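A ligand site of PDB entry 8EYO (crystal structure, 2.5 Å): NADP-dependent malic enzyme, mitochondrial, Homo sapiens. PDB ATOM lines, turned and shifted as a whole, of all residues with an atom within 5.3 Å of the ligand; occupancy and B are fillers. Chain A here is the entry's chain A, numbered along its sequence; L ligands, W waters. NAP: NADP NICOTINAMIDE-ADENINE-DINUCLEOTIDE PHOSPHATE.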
ATOM      1  N   ARG A 146     -14.756 -11.292  -9.193  1.00  0.00           N
ATOM      2  CA  ARG A 146     -13.505 -11.650  -8.518  1.00  0.00           C
ATOM      3  C   ARG A 146     -12.553 -12.334  -9.506  1.00  0.00           C
ATOM      4  O   ARG A 146     -12.221 -13.514  -9.367  1.00  0.00           O
ATOM      5  CB  ARG A 146     -13.768 -12.552  -7.312  1.00  0.00           C
ATOM      6  CG  ARG A 146     -14.325 -11.842  -6.088  1.00  0.00           C
ATOM      7  CD  ARG A 146     -13.289 -10.953  -5.410  1.00  0.00           C
ATOM      8  NE  ARG A 146     -13.602  -9.539  -5.581  1.00  0.00           N
ATOM      9  CZ  ARG A 146     -14.467  -8.871  -4.822  1.00  0.00           C
ATOM     10  NH1 ARG A 146     -15.096  -9.495  -3.831  1.00  0.00           N
ATOM     11  NH2 ARG A 146     -14.700  -7.589  -5.050  1.00  0.00           N
ATOM     12  N   LEU A 148      -9.310 -13.571 -10.666  1.00  0.00           N
ATOM     13  CA  LEU A 148      -8.202 -14.026  -9.822  1.00  0.00           C
ATOM     14  C   LEU A 148      -7.016 -13.071  -9.895  1.00  0.00           C
ATOM     15  O   LEU A 148      -6.346 -12.986 -10.926  1.00  0.00           O
ATOM     16  CB  LEU A 148      -7.753 -15.442 -10.221  1.00  0.00           C
ATOM     17  CG  LEU A 148      -6.599 -16.025  -9.396  1.00  0.00           C
ATOM     18  CD1 LEU A 148      -7.005 -17.341  -8.733  1.00  0.00           C
ATOM     19  CD2 LEU A 148      -5.355 -16.231 -10.260  1.00  0.00           C
ATOM     20  N   GLY A 149      -6.764 -12.359  -8.807  1.00  0.00           N
ATOM     21  CA  GLY A 149      -5.628 -11.466  -8.709  1.00  0.00           C
ATOM     22  C   GLY A 149      -5.897 -10.010  -9.039  1.00  0.00           C
ATOM     23  O   GLY A 149      -4.999  -9.178  -8.849  1.00  0.00           O
ATOM     24  N   ASN A 240     -17.269 -14.487  -3.106  1.00  0.00           N
ATOM     25  CA  ASN A 240     -17.293 -15.609  -2.175  1.00  0.00           C
ATOM     26  C   ASN A 240     -18.705 -16.078  -1.857  1.00  0.00           C
ATOM     27  O   ASN A 240     -19.028 -17.265  -2.009  1.00  0.00           O
ATOM     28  CB  ASN A 240     -16.550 -15.219  -0.894  1.00  0.00           C
ATOM     29  CG  ASN A 240     -16.407 -16.378   0.074  1.00  0.00           C
ATOM     30  OD1 ASN A 240     -16.735 -17.521  -0.244  1.00  0.00           O
ATOM     31  ND2 ASN A 240     -15.918 -16.091   1.279  1.00  0.00           N
ATOM     32  N   ASP A 260     -12.864 -22.314  -8.633  1.00  0.00           N
ATOM     33  CA  ASP A 260     -12.161 -21.588  -7.582  1.00  0.00           C
ATOM     34  C   ASP A 260     -12.341 -22.261  -6.225  1.00  0.00           C
ATOM     35  O   ASP A 260     -11.462 -22.170  -5.375  1.00  0.00           O
ATOM     36  CB  ASP A 260     -12.628 -20.140  -7.532  1.00  0.00           C
ATOM     37  CG  ASP A 260     -12.414 -19.413  -8.843  1.00  0.00           C
ATOM     38  OD1 ASP A 260     -13.377 -18.801  -9.354  1.00  0.00           O
ATOM     39  OD2 ASP A 260     -11.279 -19.455  -9.377  1.00  0.00           O
ATOM     40  N   THR A 264      -9.478 -25.690  -6.875  1.00  0.00           N
ATOM     41  CA  THR A 264      -8.466 -25.273  -5.909  1.00  0.00           C
ATOM     42  C   THR A 264      -8.298 -26.311  -4.805  1.00  0.00           C
ATOM     43  O   THR A 264      -7.170 -26.691  -4.462  1.00  0.00           O
ATOM     44  CB  THR A 264      -8.860 -23.928  -5.286  1.00  0.00           C
ATOM     45  OG1 THR A 264      -9.116 -22.975  -6.320  1.00  0.00           O
ATOM     46  CG2 THR A 264      -7.773 -23.432  -4.361  1.00  0.00           C
ATOM     47  N   VAL A 267      -6.360 -29.491  -6.077  1.00  0.00           N
ATOM     48  CA  VAL A 267      -4.922 -29.431  -6.303  1.00  0.00           C
ATOM     49  C   VAL A 267      -4.162 -29.168  -5.011  1.00  0.00           C
ATOM     50  O   VAL A 267      -3.021 -29.607  -4.851  1.00  0.00           O
ATOM     51  CB  VAL A 267      -4.598 -28.389  -7.391  1.00  0.00           C
ATOM     52  CG1 VAL A 267      -4.951 -26.994  -6.907  1.00  0.00           C
ATOM     53  CG2 VAL A 267      -3.130 -28.462  -7.800  1.00  0.00           C
ATOM     54  N   GLN A 291      -4.092 -19.629   6.884  1.00  0.00           N
ATOM     55  CA  GLN A 291      -3.996 -18.168   6.823  1.00  0.00           C
ATOM     56  C   GLN A 291      -4.999 -17.729   5.762  1.00  0.00           C
ATOM     57  O   GLN A 291      -4.755 -17.871   4.561  1.00  0.00           O
ATOM     58  CB  GLN A 291      -2.569 -17.727   6.507  1.00  0.00           C
ATOM     59  CG  GLN A 291      -2.435 -16.352   5.869  1.00  0.00           C
ATOM     60  CD  GLN A 291      -2.587 -15.209   6.867  1.00  0.00           C
ATOM     61  OE1 GLN A 291      -2.862 -15.431   8.045  1.00  0.00           O
ATOM     62  NE2 GLN A 291      -2.400 -13.986   6.396  1.00  0.00           N
ATOM     63  N   GLY A 292      -6.132 -17.220   6.209  1.00  0.00           N
ATOM     64  CA  GLY A 292      -7.246 -16.941   5.300  1.00  0.00           C
ATOM     65  C   GLY A 292      -8.358 -17.943   5.557  1.00  0.00           C
ATOM     66  O   GLY A 292      -8.109 -19.107   5.891  1.00  0.00           O
ATOM     67  N   ALA A 293      -9.595 -17.485   5.417  1.00  0.00           N
ATOM     68  CA  ALA A 293     -10.764 -18.302   5.699  1.00  0.00           C
ATOM     69  C   ALA A 293     -11.860 -18.027   4.684  1.00  0.00           C
ATOM     70  O   ALA A 293     -13.043 -17.955   5.029  1.00  0.00           O
ATOM     71  CB  ALA A 293     -11.271 -18.051   7.123  1.00  0.00           C
ATOM     72  N   GLY A 294     -11.483 -17.869   3.426  1.00  0.00           N
ATOM     73  CA  GLY A 294     -12.432 -17.510   2.400  1.00  0.00           C
ATOM     74  C   GLY A 294     -12.729 -18.622   1.408  1.00  0.00           C
ATOM     75  O   GLY A 294     -12.829 -19.790   1.767  1.00  0.00           O
ATOM     76  N   GLU A 295     -12.853 -18.233   0.132  1.00  0.00           N
ATOM     77  CA  GLU A 295     -13.275 -19.172  -0.910  1.00  0.00           C
ATOM     78  C   GLU A 295     -12.330 -20.352  -1.014  1.00  0.00           C
ATOM     79  O   GLU A 295     -12.759 -21.513  -1.010  1.00  0.00           O
ATOM     80  CB  GLU A 295     -13.379 -18.436  -2.249  1.00  0.00           C
ATOM     81  CG  GLU A 295     -13.953 -19.258  -3.370  1.00  0.00           C
ATOM     82  CD  GLU A 295     -14.689 -18.412  -4.404  1.00  0.00           C
ATOM     83  OE1 GLU A 295     -15.217 -17.342  -4.025  1.00  0.00           O
ATOM     84  OE2 GLU A 295     -14.740 -18.802  -5.584  1.00  0.00           O
ATOM     85  N   ALA A 296     -11.019 -20.079  -1.108  1.00  0.00           N
ATOM     86  CA  ALA A 296     -10.057 -21.166  -1.279  1.00  0.00           C
ATOM     87  C   ALA A 296      -9.896 -21.973   0.002  1.00  0.00           C
ATOM     88  O   ALA A 296      -9.798 -23.199  -0.041  1.00  0.00           O
ATOM     89  CB  ALA A 296      -8.716 -20.599  -1.742  1.00  0.00           C
ATOM     90  N   ALA A 297      -9.872 -21.294   1.158  1.00  0.00           N
ATOM     91  CA  ALA A 297      -9.688 -21.996   2.422  1.00  0.00           C
ATOM     92  C   ALA A 297     -10.820 -22.998   2.667  1.00  0.00           C
ATOM     93  O   ALA A 297     -10.569 -24.169   2.956  1.00  0.00           O
ATOM     94  CB  ALA A 297      -9.598 -20.988   3.569  1.00  0.00           C
ATOM     95  N   VAL A 325      -7.633 -18.779  10.259  1.00  0.00           N
ATOM     96  CA  VAL A 325      -7.386 -17.392  10.659  1.00  0.00           C
ATOM     97  C   VAL A 325      -7.894 -16.481   9.551  1.00  0.00           C
ATOM     98  O   VAL A 325      -7.533 -16.658   8.381  1.00  0.00           O
ATOM     99  CB  VAL A 325      -5.887 -17.143  10.922  1.00  0.00           C
ATOM    100  CG1 VAL A 325      -5.673 -15.749  11.479  1.00  0.00           C
ATOM    101  CG2 VAL A 325      -5.329 -18.201  11.875  1.00  0.00           C
ATOM    102  N   ASP A 326      -8.739 -15.524   9.912  1.00  0.00           N
ATOM    103  CA  ASP A 326      -9.234 -14.548   8.953  1.00  0.00           C
ATOM    104  C   ASP A 326      -8.716 -13.151   9.328  1.00  0.00           C
ATOM    105  O   ASP A 326      -7.772 -13.006  10.113  1.00  0.00           O
ATOM    106  CB  ASP A 326     -10.763 -14.611   8.864  1.00  0.00           C
ATOM    107  CG  ASP A 326     -11.454 -14.239  10.164  1.00  0.00           C
ATOM    108  OD1 ASP A 326     -10.760 -13.966  11.176  1.00  0.00           O
ATOM    109  OD2 ASP A 326     -12.699 -14.210  10.182  1.00  0.00           O
ATOM    110  N   SER A 327      -9.355 -12.120   8.769  1.00  0.00           N
ATOM    111  CA  SER A 327      -8.888 -10.761   8.989  1.00  0.00           C
ATOM    112  C   SER A 327      -9.134 -10.257  10.405  1.00  0.00           C
ATOM    113  O   SER A 327      -8.760  -9.123  10.717  1.00  0.00           O
ATOM    114  CB  SER A 327      -9.540  -9.803   7.986  1.00  0.00           C
ATOM    115  OG  SER A 327     -10.947  -9.723   8.192  1.00  0.00           O
ATOM    116  N   LYS A 328      -9.745 -11.072  11.277  1.00  0.00           N
ATOM    117  CA  LYS A 328      -9.980 -10.690  12.663  1.00  0.00           C
ATOM    118  C   LYS A 328      -9.208 -11.549  13.662  1.00  0.00           C
ATOM    119  O   LYS A 328      -9.237 -11.250  14.857  1.00  0.00           O
ATOM    120  CB  LYS A 328     -11.473 -10.763  12.988  1.00  0.00           C
ATOM    121  N   LYS A 342     -17.855 -20.395   8.542  1.00  0.00           N
ATOM    122  CA  LYS A 342     -16.815 -20.162   9.535  1.00  0.00           C
ATOM    123  C   LYS A 342     -17.116 -20.859  10.858  1.00  0.00           C
ATOM    124  O   LYS A 342     -16.174 -21.295  11.537  1.00  0.00           O
ATOM    125  CB  LYS A 342     -16.647 -18.660   9.760  1.00  0.00           C
ATOM    126  CG  LYS A 342     -16.270 -17.879   8.515  1.00  0.00           C
ATOM    127  CD  LYS A 342     -15.649 -16.541   8.880  1.00  0.00           C
ATOM    128  CE  LYS A 342     -15.003 -15.887   7.669  1.00  0.00           C
ATOM    129  NZ  LYS A 342     -14.197 -14.706   8.069  1.00  0.00           N
ATOM    130  N   GLY A 369      -1.366 -20.744   3.180  1.00  0.00           N
ATOM    131  CA  GLY A 369      -1.681 -19.351   2.988  1.00  0.00           C
ATOM    132  C   GLY A 369      -2.604 -19.102   1.810  1.00  0.00           C
ATOM    133  O   GLY A 369      -2.235 -19.350   0.657  1.00  0.00           O
ATOM    134  N   VAL A 370      -3.805 -18.625   2.103  1.00  0.00           N
ATOM    135  CA  VAL A 370      -4.778 -18.294   1.056  1.00  0.00           C
ATOM    136  C   VAL A 370      -5.493 -17.009   1.459  1.00  0.00           C
ATOM    137  O   VAL A 370      -6.720 -16.909   1.357  1.00  0.00           O
ATOM    138  CB  VAL A 370      -5.780 -19.449   0.840  1.00  0.00           C
ATOM    139  CG1 VAL A 370      -5.180 -20.498  -0.080  1.00  0.00           C
ATOM    140  CG2 VAL A 370      -6.173 -20.061   2.174  1.00  0.00           C
ATOM    141  N   ALA A 371      -4.727 -16.019   1.931  1.00  0.00           N
ATOM    142  CA  ALA A 371      -5.282 -14.762   2.400  1.00  0.00           C
ATOM    143  C   ALA A 371      -4.814 -13.561   1.595  1.00  0.00           C
ATOM    144  O   ALA A 371      -5.339 -12.458   1.804  1.00  0.00           O
ATOM    145  CB  ALA A 371      -4.931 -14.539   3.877  1.00  0.00           C
ATOM    146  N   ALA A 372      -3.841 -13.730   0.702  1.00  0.00           N
ATOM    147  CA  ALA A 372      -3.330 -12.663  -0.159  1.00  0.00           C
ATOM    148  C   ALA A 372      -2.686 -11.550   0.665  1.00  0.00           C
ATOM    149  O   ALA A 372      -2.782 -10.365   0.326  1.00  0.00           O
ATOM    150  CB  ALA A 372      -4.425 -12.106  -1.073  1.00  0.00           C
ATOM    151  N   ILE A 373      -2.009 -11.926   1.753  1.00  0.00           N
ATOM    152  CA  ILE A 373      -1.231 -10.987   2.562  1.00  0.00           C
ATOM    153  C   ILE A 373       0.231 -11.350   2.370  1.00  0.00           C
ATOM    154  O   ILE A 373       0.679 -12.428   2.762  1.00  0.00           O
ATOM    155  CB  ILE A 373      -1.631 -11.031   4.034  1.00  0.00           C
ATOM    156  CG1 ILE A 373      -3.142 -10.837   4.192  1.00  0.00           C
ATOM    157  CG2 ILE A 373      -0.883  -9.945   4.809  1.00  0.00           C
ATOM    158  CD1 ILE A 373      -3.650  -9.508   3.657  1.00  0.00           C
ATOM    159  N   LEU A 397       0.041 -20.119  -1.168  1.00  0.00           N
ATOM    160  CA  LEU A 397      -0.792 -20.240  -2.352  1.00  0.00           C
ATOM    161  C   LEU A 397      -1.304 -18.902  -2.891  1.00  0.00           C
ATOM    162  O   LEU A 397      -1.896 -18.878  -3.968  1.00  0.00           O
ATOM    163  CB  LEU A 397      -1.996 -21.157  -2.060  1.00  0.00           C
ATOM    164  CG  LEU A 397      -1.607 -22.541  -1.552  1.00  0.00           C
ATOM    165  CD1 LEU A 397      -2.820 -23.457  -1.444  1.00  0.00           C
ATOM    166  CD2 LEU A 397      -0.540 -23.156  -2.447  1.00  0.00           C
ATOM    167  N   SER A 398      -1.073 -17.796  -2.186  1.00  0.00           N
ATOM    168  CA  SER A 398      -1.636 -16.518  -2.603  1.00  0.00           C
ATOM    169  C   SER A 398      -0.995 -16.025  -3.894  1.00  0.00           C
ATOM    170  O   SER A 398       0.208 -16.146  -4.098  1.00  0.00           O
ATOM    171  CB  SER A 398      -1.458 -15.481  -1.491  1.00  0.00           C
ATOM    172  OG  SER A 398      -2.339 -15.739  -0.414  1.00  0.00           O
ATOM    173  N   ASN A 399      -1.840 -15.461  -4.763  1.00  0.00           N
ATOM    174  CA  ASN A 399      -1.439 -14.920  -6.055  1.00  0.00           C
ATOM    175  C   ASN A 399      -1.797 -13.439  -6.136  1.00  0.00           C
ATOM    176  O   ASN A 399      -2.774 -12.998  -5.521  1.00  0.00           O
ATOM    177  CB  ASN A 399      -2.128 -15.678  -7.199  1.00  0.00           C
ATOM    178  CG  ASN A 399      -1.612 -17.095  -7.355  1.00  0.00           C
ATOM    179  OD1 ASN A 399      -0.415 -17.327  -7.519  1.00  0.00           O
ATOM    180  ND2 ASN A 399      -2.522 -18.065  -7.288  1.00  0.00           N
ATOM    181  N   SER A 423       3.660 -23.348  -3.979  1.00  0.00           N
ATOM    182  CA  SER A 423       3.147 -21.998  -4.153  1.00  0.00           C
ATOM    183  C   SER A 423       2.063 -21.995  -5.229  1.00  0.00           C
ATOM    184  O   SER A 423       1.871 -22.971  -5.958  1.00  0.00           O
ATOM    185  CB  SER A 423       4.263 -21.024  -4.533  1.00  0.00           C
ATOM    186  OG  SER A 423       4.970 -21.474  -5.678  1.00  0.00           O
ATOM    187  N   GLY A 424       1.348 -20.884  -5.304  1.00  0.00           N
ATOM    188  CA  GLY A 424       0.378 -20.682  -6.359  1.00  0.00           C
ATOM    189  C   GLY A 424       1.023 -20.035  -7.558  1.00  0.00           C
ATOM    190  O   GLY A 424       0.625 -20.266  -8.706  1.00  0.00           O
ATOM    191  N   GLY A 443       0.992 -25.192  -7.430  1.00  0.00           N
ATOM    192  CA  GLY A 443      -0.299 -25.825  -7.339  1.00  0.00           C
ATOM    193  C   GLY A 443      -1.282 -25.281  -8.360  1.00  0.00           C
ATOM    194  O   GLY A 443      -2.196 -24.517  -8.016  1.00  0.00           O
ATOM    195  N   ASN A 444      -1.095 -25.664  -9.622  1.00  0.00           N
ATOM    196  CA  ASN A 444      -1.862 -25.105 -10.715  1.00  0.00           C
ATOM    197  C   ASN A 444      -3.214 -25.793 -10.842  1.00  0.00           C
ATOM    198  O   ASN A 444      -3.300 -27.023 -10.841  1.00  0.00           O
ATOM    199  CB  ASN A 444      -1.076 -25.241 -12.025  1.00  0.00           C
ATOM    200  CG  ASN A 444      -1.480 -24.219 -13.068  1.00  0.00           C
ATOM    201  OD1 ASN A 444      -2.666 -24.046 -13.360  1.00  0.00           O
ATOM    202  ND2 ASN A 444      -0.491 -23.526 -13.627  1.00  0.00           N
ATOM    203  N   ASN A 445      -4.285 -24.989 -10.957  1.00  0.00           N
ATOM    204  CA  ASN A 445      -5.620 -25.555 -11.083  1.00  0.00           C
ATOM    205  C   ASN A 445      -5.763 -26.384 -12.355  1.00  0.00           C
ATOM    206  O   ASN A 445      -6.591 -27.296 -12.416  1.00  0.00           O
ATOM    207  CB  ASN A 445      -6.667 -24.450 -11.039  1.00  0.00           C
ATOM    208  CG  ASN A 445      -7.027 -24.040  -9.639  1.00  0.00           C
ATOM    209  OD1 ASN A 445      -6.170 -23.979  -8.760  1.00  0.00           O
ATOM    210  ND2 ASN A 445      -8.299 -23.753  -9.413  1.00  0.00           N
HETATM  211  PA  NAP L   1     -11.326 -14.499  -0.573  1.00  0.00           P
HETATM  212  O1A NAP L   1     -12.323 -15.594  -0.288  1.00  0.00           O
HETATM  213  O2A NAP L   1     -12.057 -13.258  -1.038  1.00  0.00           O
HETATM  214  O5B NAP L   1     -10.466 -14.123   0.794  1.00  0.00           O
HETATM  215  C5B NAP L   1      -9.750 -15.124   1.465  1.00  0.00           C
HETATM  216  C4B NAP L   1      -9.459 -14.745   2.959  1.00  0.00           C
HETATM  217  O4B NAP L   1      -8.469 -13.907   3.109  1.00  0.00           O
HETATM  218  C3B NAP L   1     -10.660 -14.023   3.622  1.00  0.00           C
HETATM  219  O3B NAP L   1     -11.318 -14.894   4.427  1.00  0.00           O
HETATM  220  C2B NAP L   1     -10.012 -12.919   4.475  1.00  0.00           C
HETATM  221  O2B NAP L   1     -10.632 -12.843   5.825  1.00  0.00           O
HETATM  222  C1B NAP L   1      -8.776 -13.323   4.580  1.00  0.00           C
HETATM  223  N9A NAP L   1      -7.916 -12.237   5.007  1.00  0.00           N
HETATM  224  C8A NAP L   1      -7.862 -10.975   4.555  1.00  0.00           C
HETATM  225  N7A NAP L   1      -6.923 -10.330   5.255  1.00  0.00           N
HETATM  226  C5A NAP L   1      -6.405 -11.177   6.145  1.00  0.00           C
HETATM  227  C6A NAP L   1      -5.417 -11.037   7.100  1.00  0.00           C
HETATM  228  N6A NAP L   1      -4.572  -9.938   7.516  1.00  0.00           N
HETATM  229  N1A NAP L   1      -5.076 -12.058   7.867  1.00  0.00           N
HETATM  230  C2A NAP L   1      -5.696 -13.253   7.713  1.00  0.00           C
HETATM  231  N3A NAP L   1      -6.666 -13.399   6.781  1.00  0.00           N
HETATM  232  C4A NAP L   1      -7.020 -12.358   5.991  1.00  0.00           C
HETATM  233  O3  NAP L   1     -10.315 -14.949  -1.794  1.00  0.00           O
HETATM  234  PN  NAP L   1      -9.916 -16.496  -2.245  1.00  0.00           P
HETATM  235  O1N NAP L   1     -10.708 -16.931  -3.453  1.00  0.00           O
HETATM  236  O2N NAP L   1     -10.111 -17.473  -1.114  1.00  0.00           O
HETATM  237  O5D NAP L   1      -8.323 -16.458  -2.633  1.00  0.00           O
HETATM  238  C5D NAP L   1      -7.438 -16.080  -1.620  1.00  0.00           C
HETATM  239  C4D NAP L   1      -6.014 -16.398  -2.139  1.00  0.00           C
HETATM  240  O4D NAP L   1      -5.953 -17.647  -2.508  1.00  0.00           O
HETATM  241  C3D NAP L   1      -5.807 -15.541  -3.407  1.00  0.00           C
HETATM  242  O3D NAP L   1      -4.621 -14.883  -3.341  1.00  0.00           O
HETATM  243  C2D NAP L   1      -5.811 -16.565  -4.558  1.00  0.00           C
HETATM  244  O2D NAP L   1      -4.943 -16.112  -5.679  1.00  0.00           O
HETATM  245  C1D NAP L   1      -5.322 -17.640  -3.999  1.00  0.00           C
HETATM  246  N1N NAP L   1      -5.718 -18.806  -4.757  1.00  0.00           N
HETATM  247  C2N NAP L   1      -4.758 -19.652  -5.200  1.00  0.00           C
HETATM  248  C3N NAP L   1      -5.113 -20.773  -5.941  1.00  0.00           C
HETATM  249  C7N NAP L   1      -4.032 -21.735  -6.442  1.00  0.00           C
HETATM  250  O7N NAP L   1      -2.901 -21.606  -6.086  1.00  0.00           O
HETATM  251  N7N NAP L   1      -4.375 -22.818  -7.350  1.00  0.00           N
HETATM  252  C4N NAP L   1      -6.412 -21.010  -6.214  1.00  0.00           C
HETATM  253  C5N NAP L   1      -7.374 -20.171  -5.760  1.00  0.00           C
HETATM  254  C6N NAP L   1      -7.014 -19.052  -5.027  1.00  0.00           C
HETATM  255  P2B NAP L   1     -12.139 -12.186   5.994  1.00  0.00           P
HETATM  256  O1X NAP L   1     -12.279 -10.977   5.089  1.00  0.00           O
HETATM  257  O2X NAP L   1     -13.183 -13.217   5.646  1.00  0.00           O
HETATM  258  O3X NAP L   1     -12.340 -11.751   7.426  1.00  0.00           O
HETATM  259  O   HOH W   1      -9.544 -18.366   1.261  1.00  0.00           O
HETATM  260  O   HOH W   2      -2.138  -9.777  10.001  1.00  0.00           O
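NZ of Lys 342 is in salt-bridge range of O2X of the ligand.
The side-chain amide oxygen of Asn 445 sits at hydrogen-bond distance from a nitrogen (N7N) of the ligand, 2.6 Å away.
The backbone carbonyl oxygen (O) of Gly 443 is in hydrogen-bond range of a nitrogen (N7N) of the ligand (2.8 Å).
O2B of the ligand lies within hydrogen-bond range of N of Ser 327.
The side-chain hydroxyl of Ser 327 is in hydrogen-bond range of an oxygen (O3X) of the ligand (2.6 Å).
An oxygen (O1A) of the ligand is in hydrogen-bond range of the backbone NH (N) of Glu 295.
N of Asn 399 is in hydrogen-bond range of O3D of the ligand (3.2 Å).
The backbone NH (N) of Ala 293 sits close to an oxygen (O3B) of the ligand.
An oxygen (O2N) of the ligand sits at hydrogen-bond distance from the backbone NH of Ala 296 (2.8 Å).
An oxygen (O3B) of the ligand lies within hydrogen-bond range of the backbone NH (N) of Gly 294 (3.1 Å).
O of Asn 399 sits at hydrogen-bond distance from O3D of the ligand (3.4 Å).
The backbone carbonyl oxygen of Gly 424 sits close to the side-chain amide oxygen of Asn 399 (3.3 Å).
O of Asp 260 is in hydrogen-bond range of OG1 of Thr 264, at 2.7 Å.
N of Lys 328 lies close to OD1 of Asp 326 (3.1 Å).
The side-chain amino group (NZ) of Lys 342 lies within salt-bridge range of the side-chain carboxylate (OD2) of Asp 326, at 2.6 Å.
N of Gly 292 is in hydrogen-bond range of O of Val 325 (2.6 Å).
O of Gln 291 lies within hydrogen-bond range of N of Ala 371 (3.2 Å).
The side-chain hydroxyl (OG) of Ser 398 is in hydrogen-bond range of the backbone NH (N) of Ala 371.
O of Leu 397 is in hydrogen-bond range of ND2 of Asn 399 (3.5 Å).
Residues that only touch the ligand: Leu 148 (3.9 Å), Asn 240 (3.95 Å), Thr 264 (3.3 Å), Gln 291 (3.6 Å), Gly 292 (3.9 Å), Val 325 (3.7 Å), Asp 326 (3.2 Å), Val 370 (3.2 Å), Ala 371 (3.4 Å), Ala 372 (3.6 Å), Ile 373 (3.7 Å), Leu 397 (3.2 Å), Ser 398 (3.5 Å) and Gly 424 (3.4 Å).
Hydrophobic or aromatic side chains that line the ligand: Leu 148, Ala 296, Val 370, Ala 371, Ala 372 and Ile 373.
Within 4 Å of the ligand: Leu 148, Asn 240, Thr 264, Gln 291, Gly 292, Ala 293, Gly 294, Glu 295, Ala 296, Val 325, Asp 326, Ser 327, Lys 342, Val 370, Ala 371, Ala 372, Ile 373, Leu 397, Ser 398, Asn 399, Gly 424, Gly 443 and Asn 445.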
